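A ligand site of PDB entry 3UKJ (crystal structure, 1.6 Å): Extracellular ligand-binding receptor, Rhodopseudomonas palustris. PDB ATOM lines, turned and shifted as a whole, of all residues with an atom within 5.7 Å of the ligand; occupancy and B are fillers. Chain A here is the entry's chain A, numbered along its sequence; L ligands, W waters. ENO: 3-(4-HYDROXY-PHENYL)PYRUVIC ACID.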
ATOM      1  N   LEU A  23       6.629   1.172  10.388  1.00  0.00           N
ATOM      2  CA  LEU A  23       6.936   0.119  11.372  1.00  0.00           C
ATOM      3  C   LEU A  23       5.697  -0.767  11.634  1.00  0.00           C
ATOM      4  O   LEU A  23       5.801  -1.993  11.628  1.00  0.00           O
ATOM      5  CB  LEU A  23       7.510   0.737  12.665  1.00  0.00           C
ATOM      6  CG  LEU A  23       9.009   1.074  12.670  1.00  0.00           C
ATOM      7  CD1 LEU A  23       9.367   2.170  11.665  1.00  0.00           C
ATOM      8  CD2 LEU A  23       9.441   1.488  14.065  1.00  0.00           C
ATOM      9  N   GLU A  27       4.186  -4.950  10.680  1.00  0.00           N
ATOM     10  CA  GLU A  27       3.731  -5.677  11.881  1.00  0.00           C
ATOM     11  C   GLU A  27       2.317  -6.233  11.728  1.00  0.00           C
ATOM     12  O   GLU A  27       2.088  -7.423  11.959  1.00  0.00           O
ATOM     13  CB  GLU A  27       3.861  -4.808  13.128  1.00  0.00           C
ATOM     14  CG  GLU A  27       5.330  -4.677  13.497  1.00  0.00           C
ATOM     15  CD  GLU A  27       5.691  -3.599  14.503  1.00  0.00           C
ATOM     16  OE1 GLU A  27       4.808  -2.840  14.973  1.00  0.00           O
ATOM     17  OE2 GLU A  27       6.910  -3.508  14.777  1.00  0.00           O
ATOM     18  N   SER A  77       3.987   0.131  18.048  1.00  0.00           N
ATOM     19  CA  SER A  77       5.086   0.110  17.082  1.00  0.00           C
ATOM     20  C   SER A  77       6.279   0.976  17.420  1.00  0.00           C
ATOM     21  O   SER A  77       7.387   0.731  16.919  1.00  0.00           O
ATOM     22  CB  SER A  77       4.562   0.484  15.687  1.00  0.00           C
ATOM     23  OG  SER A  77       3.536  -0.416  15.268  1.00  0.00           O
ATOM     24  N   VAL A  78       6.067   1.957  18.275  1.00  0.00           N
ATOM     25  CA  VAL A  78       7.129   2.862  18.735  1.00  0.00           C
ATOM     26  C   VAL A  78       7.015   3.035  20.264  1.00  0.00           C
ATOM     27  O   VAL A  78       6.043   2.582  20.889  1.00  0.00           O
ATOM     28  CB  VAL A  78       7.127   4.206  17.957  1.00  0.00           C
ATOM     29  CG1 VAL A  78       7.627   3.952  16.503  1.00  0.00           C
ATOM     30  CG2 VAL A  78       5.742   4.831  17.968  1.00  0.00           C
ATOM     31  N   THR A  79       8.037   3.602  20.865  1.00  0.00           N
ATOM     32  CA  THR A  79       8.191   3.525  22.314  1.00  0.00           C
ATOM     33  C   THR A  79       7.073   4.243  23.106  1.00  0.00           C
ATOM     34  O   THR A  79       6.509   3.643  24.052  1.00  0.00           O
ATOM     35  CB  THR A  79       9.618   3.994  22.717  1.00  0.00           C
ATOM     36  OG1 THR A  79      10.562   3.066  22.160  1.00  0.00           O
ATOM     37  CG2 THR A  79       9.792   3.949  24.235  1.00  0.00           C
ATOM     38  N   PRO A  80       6.690   5.479  22.689  1.00  0.00           N
ATOM     39  CA  PRO A  80       5.700   6.164  23.548  1.00  0.00           C
ATOM     40  C   PRO A  80       4.359   5.430  23.703  1.00  0.00           C
ATOM     41  O   PRO A  80       3.914   5.238  24.829  1.00  0.00           O
ATOM     42  CB  PRO A  80       5.543   7.555  22.924  1.00  0.00           C
ATOM     43  CG  PRO A  80       6.874   7.808  22.219  1.00  0.00           C
ATOM     44  CD  PRO A  80       7.326   6.406  21.719  1.00  0.00           C
ATOM     45  N   LEU A  99       6.031  -4.570  21.009  1.00  0.00           N
ATOM     46  CA  LEU A  99       6.672  -4.648  19.693  1.00  0.00           C
ATOM     47  C   LEU A  99       7.685  -3.521  19.439  1.00  0.00           C
ATOM     48  O   LEU A  99       8.249  -3.406  18.323  1.00  0.00           O
ATOM     49  CB  LEU A  99       5.628  -4.748  18.583  1.00  0.00           C
ATOM     50  CG  LEU A  99       4.576  -5.883  18.688  1.00  0.00           C
ATOM     51  CD1 LEU A  99       3.643  -5.805  17.496  1.00  0.00           C
ATOM     52  CD2 LEU A  99       5.320  -7.263  18.797  1.00  0.00           C
ATOM     53  N   ALA A 100       7.910  -2.676  20.454  1.00  0.00           N
ATOM     54  CA  ALA A 100       8.942  -1.611  20.418  1.00  0.00           C
ATOM     55  C   ALA A 100       9.729  -1.678  21.737  1.00  0.00           C
ATOM     56  O   ALA A 100       9.156  -2.076  22.769  1.00  0.00           O
ATOM     57  CB  ALA A 100       8.276  -0.193  20.272  1.00  0.00           C
ATOM     58  N   PRO A 101      11.017  -1.282  21.717  1.00  0.00           N
ATOM     59  CA  PRO A 101      11.747  -1.287  22.979  1.00  0.00           C
ATOM     60  C   PRO A 101      11.158  -0.231  23.924  1.00  0.00           C
ATOM     61  O   PRO A 101      10.411   0.691  23.499  1.00  0.00           O
ATOM     62  CB  PRO A 101      13.171  -0.863  22.582  1.00  0.00           C
ATOM     63  CG  PRO A 101      13.150  -0.551  21.144  1.00  0.00           C
ATOM     64  CD  PRO A 101      11.848  -0.936  20.561  1.00  0.00           C
ATOM     65  N   PRO A 116      11.482  -6.583  20.473  1.00  0.00           N
ATOM     66  CA  PRO A 116      12.737  -6.022  19.930  1.00  0.00           C
ATOM     67  C   PRO A 116      13.906  -6.179  20.866  1.00  0.00           C
ATOM     68  O   PRO A 116      13.744  -6.164  22.091  1.00  0.00           O
ATOM     69  CB  PRO A 116      12.440  -4.534  19.770  1.00  0.00           C
ATOM     70  CG  PRO A 116      11.057  -4.364  19.984  1.00  0.00           C
ATOM     71  CD  PRO A 116      10.377  -5.609  20.399  1.00  0.00           C
ATOM     72  N   GLN A 117      15.101  -6.107  20.281  1.00  0.00           N
ATOM     73  CA  GLN A 117      16.340  -6.281  21.056  1.00  0.00           C
ATOM     74  C   GLN A 117      16.512  -5.067  21.990  1.00  0.00           C
ATOM     75  O   GLN A 117      16.088  -3.949  21.629  1.00  0.00           O
ATOM     76  CB  GLN A 117      17.519  -6.328  20.106  1.00  0.00           C
ATOM     77  CG  GLN A 117      17.575  -7.621  19.250  1.00  0.00           C
ATOM     78  CD  GLN A 117      16.691  -7.604  18.013  1.00  0.00           C
ATOM     79  OE1 GLN A 117      16.088  -6.578  17.663  1.00  0.00           O
ATOM     80  NE2 GLN A 117      16.556  -8.792  17.376  1.00  0.00           N
ATOM     81  N   TYR A 143      15.508  11.221  18.868  1.00  0.00           N
ATOM     82  CA  TYR A 143      14.233  11.778  19.339  1.00  0.00           C
ATOM     83  C   TYR A 143      14.340  12.436  20.704  1.00  0.00           C
ATOM     84  O   TYR A 143      15.019  11.921  21.624  1.00  0.00           O
ATOM     85  CB  TYR A 143      13.116  10.726  19.387  1.00  0.00           C
ATOM     86  CG  TYR A 143      12.840  10.065  18.083  1.00  0.00           C
ATOM     87  CD1 TYR A 143      12.646  10.819  16.892  1.00  0.00           C
ATOM     88  CD2 TYR A 143      12.581   8.696  18.042  1.00  0.00           C
ATOM     89  CE1 TYR A 143      12.364  10.171  15.700  1.00  0.00           C
ATOM     90  CE2 TYR A 143      12.154   8.077  16.884  1.00  0.00           C
ATOM     91  CZ  TYR A 143      12.034   8.826  15.720  1.00  0.00           C
ATOM     92  OH  TYR A 143      11.650   8.206  14.573  1.00  0.00           O
ATOM     93  N   ASP A 145      12.417  11.995  23.194  1.00  0.00           N
ATOM     94  CA  ASP A 145      11.487  11.191  23.985  1.00  0.00           C
ATOM     95  C   ASP A 145      12.220   9.977  24.556  1.00  0.00           C
ATOM     96  O   ASP A 145      13.416   9.890  24.427  1.00  0.00           O
ATOM     97  CB  ASP A 145      10.222  10.838  23.202  1.00  0.00           C
ATOM     98  CG  ASP A 145      10.474   9.908  22.019  1.00  0.00           C
ATOM     99  OD1 ASP A 145      11.394   9.081  22.031  1.00  0.00           O
ATOM    100  OD2 ASP A 145       9.712  10.011  21.059  1.00  0.00           O
ATOM    101  N   TYR A 147      12.601   6.880  23.701  1.00  0.00           N
ATOM    102  CA  TYR A 147      13.421   6.101  22.750  1.00  0.00           C
ATOM    103  C   TYR A 147      14.793   6.792  22.570  1.00  0.00           C
ATOM    104  O   TYR A 147      15.825   6.156  22.710  1.00  0.00           O
ATOM    105  CB  TYR A 147      12.746   5.902  21.389  1.00  0.00           C
ATOM    106  CG  TYR A 147      13.579   5.054  20.439  1.00  0.00           C
ATOM    107  CD1 TYR A 147      13.711   3.673  20.649  1.00  0.00           C
ATOM    108  CD2 TYR A 147      14.281   5.623  19.372  1.00  0.00           C
ATOM    109  CE1 TYR A 147      14.414   2.852  19.754  1.00  0.00           C
ATOM    110  CE2 TYR A 147      15.076   4.808  18.497  1.00  0.00           C
ATOM    111  CZ  TYR A 147      15.098   3.426  18.675  1.00  0.00           C
ATOM    112  OH  TYR A 147      15.843   2.600  17.876  1.00  0.00           O
ATOM    113  N   ARG A 174       9.606  13.572  16.762  1.00  0.00           N
ATOM    114  CA  ARG A 174       9.142  12.599  15.743  1.00  0.00           C
ATOM    115  C   ARG A 174       8.524  13.189  14.482  1.00  0.00           C
ATOM    116  O   ARG A 174       8.765  12.675  13.386  1.00  0.00           O
ATOM    117  CB  ARG A 174       8.199  11.551  16.335  1.00  0.00           C
ATOM    118  CG  ARG A 174       8.908  10.530  17.158  1.00  0.00           C
ATOM    119  CD  ARG A 174       7.904   9.690  17.879  1.00  0.00           C
ATOM    120  NE  ARG A 174       8.598   8.928  18.892  1.00  0.00           N
ATOM    121  CZ  ARG A 174       9.234   7.792  18.657  1.00  0.00           C
ATOM    122  NH1 ARG A 174       8.994   7.112  17.513  1.00  0.00           N
ATOM    123  NH2 ARG A 174       9.949   7.266  19.637  1.00  0.00           N
ATOM    124  N   ALA A 198      16.795   7.095  16.072  1.00  0.00           N
ATOM    125  CA  ALA A 198      15.496   7.331  15.516  1.00  0.00           C
ATOM    126  C   ALA A 198      15.025   6.043  14.862  1.00  0.00           C
ATOM    127  O   ALA A 198      15.573   4.963  15.136  1.00  0.00           O
ATOM    128  CB  ALA A 198      15.528   8.514  14.490  1.00  0.00           C
ATOM    129  N   SER A 199      13.985   6.161  14.056  1.00  0.00           N
ATOM    130  CA  SER A 199      13.390   4.981  13.448  1.00  0.00           C
ATOM    131  C   SER A 199      12.670   5.317  12.176  1.00  0.00           C
ATOM    132  O   SER A 199      12.290   6.480  11.963  1.00  0.00           O
ATOM    133  CB  SER A 199      12.414   4.280  14.435  1.00  0.00           C
ATOM    134  OG  SER A 199      11.296   5.105  14.698  1.00  0.00           O
ATOM    135  N   THR A 222      20.365   2.794  14.529  1.00  0.00           N
ATOM    136  CA  THR A 222      19.743   1.815  15.409  1.00  0.00           C
ATOM    137  C   THR A 222      18.961   0.793  14.625  1.00  0.00           C
ATOM    138  O   THR A 222      18.694   0.981  13.430  1.00  0.00           O
ATOM    139  CB  THR A 222      18.813   2.485  16.461  1.00  0.00           C
ATOM    140  OG1 THR A 222      17.604   2.932  15.846  1.00  0.00           O
ATOM    141  CG2 THR A 222      19.536   3.687  17.160  1.00  0.00           C
ATOM    142  N   HIS A 223      18.435  -0.186  15.335  1.00  0.00           N
ATOM    143  CA  HIS A 223      17.588  -1.213  14.737  1.00  0.00           C
ATOM    144  C   HIS A 223      16.168  -0.709  14.327  1.00  0.00           C
ATOM    145  O   HIS A 223      15.408  -1.377  13.638  1.00  0.00           O
ATOM    146  CB  HIS A 223      17.587  -2.514  15.567  1.00  0.00           C
ATOM    147  CG  HIS A 223      17.208  -2.338  17.009  1.00  0.00           C
ATOM    148  ND1 HIS A 223      17.673  -1.310  17.800  1.00  0.00           N
ATOM    149  CD2 HIS A 223      16.489  -3.144  17.835  1.00  0.00           C
ATOM    150  CE1 HIS A 223      17.243  -1.467  19.038  1.00  0.00           C
ATOM    151  NE2 HIS A 223      16.529  -2.584  19.089  1.00  0.00           N
ATOM    152  N   GLY A 224      15.856   0.499  14.778  1.00  0.00           N
ATOM    153  CA  GLY A 224      14.680   1.226  14.344  1.00  0.00           C
ATOM    154  C   GLY A 224      14.702   1.595  12.890  1.00  0.00           C
ATOM    155  O   GLY A 224      13.667   2.031  12.355  1.00  0.00           O
ATOM    156  N   GLN A 282      12.818  -5.715  10.075  1.00  0.00           N
ATOM    157  CA  GLN A 282      12.966  -5.884  11.501  1.00  0.00           C
ATOM    158  C   GLN A 282      11.556  -6.055  12.143  1.00  0.00           C
ATOM    159  O   GLN A 282      11.398  -6.862  13.060  1.00  0.00           O
ATOM    160  CB  GLN A 282      13.634  -4.588  12.035  1.00  0.00           C
ATOM    161  CG  GLN A 282      13.722  -4.418  13.534  1.00  0.00           C
ATOM    162  CD  GLN A 282      14.835  -5.234  14.132  1.00  0.00           C
ATOM    163  OE1 GLN A 282      15.598  -5.870  13.414  1.00  0.00           O
ATOM    164  NE2 GLN A 282      14.936  -5.235  15.449  1.00  0.00           N
ATOM    165  N   PHE A 283      10.579  -5.268  11.662  1.00  0.00           N
ATOM    166  CA  PHE A 283       9.332  -5.066  12.365  1.00  0.00           C
ATOM    167  C   PHE A 283       8.401  -6.243  12.104  1.00  0.00           C
ATOM    168  O   PHE A 283       7.703  -6.707  13.030  1.00  0.00           O
ATOM    169  CB  PHE A 283       8.725  -3.704  11.936  1.00  0.00           C
ATOM    170  CG  PHE A 283       9.757  -2.599  11.943  1.00  0.00           C
ATOM    171  CD1 PHE A 283      10.401  -2.230  13.128  1.00  0.00           C
ATOM    172  CD2 PHE A 283      10.225  -2.084  10.733  1.00  0.00           C
ATOM    173  CE1 PHE A 283      11.523  -1.397  13.107  1.00  0.00           C
ATOM    174  CE2 PHE A 283      11.264  -1.141  10.718  1.00  0.00           C
ATOM    175  CZ  PHE A 283      11.973  -0.878  11.900  1.00  0.00           C
ATOM    176  N   HIS A 286       8.988  -8.893  14.564  1.00  0.00           N
ATOM    177  CA  HIS A 286       8.476  -8.820  15.924  1.00  0.00           C
ATOM    178  C   HIS A 286       7.066  -9.372  16.096  1.00  0.00           C
ATOM    179  O   HIS A 286       6.834 -10.092  17.021  1.00  0.00           O
ATOM    180  CB  HIS A 286       8.573  -7.419  16.472  1.00  0.00           C
ATOM    181  CG  HIS A 286       9.956  -6.877  16.424  1.00  0.00           C
ATOM    182  ND1 HIS A 286      11.064  -7.656  16.726  1.00  0.00           N
ATOM    183  CD2 HIS A 286      10.429  -5.645  16.152  1.00  0.00           C
ATOM    184  CE1 HIS A 286      12.153  -6.899  16.638  1.00  0.00           C
ATOM    185  NE2 HIS A 286      11.796  -5.691  16.235  1.00  0.00           N
HETATM  186  O4  ENO L   1      10.823   2.070  19.421  1.00  0.00           O
HETATM  187  C9  ENO L   1      10.995  -0.431  16.966  1.00  0.00           C
HETATM  188  C8  ENO L   1      11.445  -1.763  16.941  1.00  0.00           C
HETATM  189  C7  ENO L   1      12.817  -1.986  17.058  1.00  0.00           C
HETATM  190  C6  ENO L   1      13.742  -0.938  17.204  1.00  0.00           C
HETATM  191  C5  ENO L   1      13.288   0.363  17.325  1.00  0.00           C
HETATM  192  C4  ENO L   1      11.920   0.630  17.143  1.00  0.00           C
HETATM  193  O3  ENO L   1      13.296  -3.255  16.947  1.00  0.00           O
HETATM  194  C3  ENO L   1      11.480   2.070  17.078  1.00  0.00           C
HETATM  195  C2  ENO L   1      11.071   2.724  18.388  1.00  0.00           C
HETATM  196  C1  ENO L   1      10.704   4.146  18.355  1.00  0.00           C
HETATM  197  O2  ENO L   1      10.259   4.613  19.393  1.00  0.00           O
HETATM  198  O1  ENO L   1      10.864   4.860  17.335  1.00  0.00           O
HETATM  199  O   HOH W   1       7.987  -1.788  16.219  1.00  0.00           O
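Leu 23 touches the ligand.
Ser 77 touches the ligand.
Val 78 touches the ligand (CG1 to O1, 3.5 Å).
Leu 99 touches the ligand (O to C8, 3.9 Å).
Ala 100 touches the ligand.
Pro 101 touches the ligand (CD to O4, 3.4 Å).
Pro 116 touches the ligand (CB to O3, 3.2 Å).
CE2 of Tyr 143 touches O1 of the ligand (3.5 Å).
Tyr 147 touches the ligand (CB to O2, 3.4 Å).
His 223 touches the ligand (CD2 to O3, 3.3 Å).
Gly 224 touches the ligand.
Phe 283 touches the ligand.
Hydrophobic or aromatic side chains that line the ligand: Leu 23, Val 78, Ala 100, Pro 101, Pro 116, Tyr 143, Tyr 147, His 223, Phe 283 and His 286.
Within 4 Å of the ligand: Leu 23, Ser 77, Val 78, Thr 79, Leu 99, Ala 100, Pro 101, Pro 116, Tyr 143, Tyr 147, Arg 174, Ser 199, His 223, Gly 224, Gln 282, Phe 283 and His 286.
The nearest printed residue that does not touch the ligand is Pro 80 (4.2 Å).
The backbone carbonyl oxygen (O) of Pro 101 lies within hydrogen-bond range of the side-chain hydroxyl (OG1) of Thr 79 (2.7 Å).
OE1 of Glu 27 is in hydrogen-bond range of OG of Ser 77 (2.8 Å).
OH of Tyr 147 lies within hydrogen-bond range of OG1 of Thr 222, at 2.7 Å.
NE2 of His 286 lies within hydrogen-bond range of NE2 of Gln 282 (3.3 Å).
The side-chain hydroxyl of Ser 199 lies within hydrogen-bond range of the side-chain hydroxyl of Tyr 143.
The side-chain carboxylate of Asp 145 sits at hydrogen-bond distance from the backbone NH of Tyr 147 (3.0 Å).
NE of Arg 174 lies within salt-bridge range of OD2 of Asp 145 (2.7 Å).
O of Gln 117 lies within hydrogen-bond range of NE2 of His 223 (2.9 Å).
The side-chain hydroxyl of Ser 199 sits at hydrogen-bond distance from an oxygen (O1) of the ligand.
An oxygen (O2) of the ligand lies within salt-bridge range of the guanidinium group of Arg 174 (2.7 Å).
The side-chain hydroxyl (OG1) of Thr 79 is in hydrogen-bond range of an oxygen (O4) of the ligand (2.9 Å).
NE2 of His 286 lies within hydrogen-bond range of O3 of the ligand (2.9 Å).
NE2 of Gln 282 lies within hydrogen-bond range of O3 of the ligand.
N of Thr 79 is in hydrogen-bond range of O2 of the ligand (2.9 Å).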
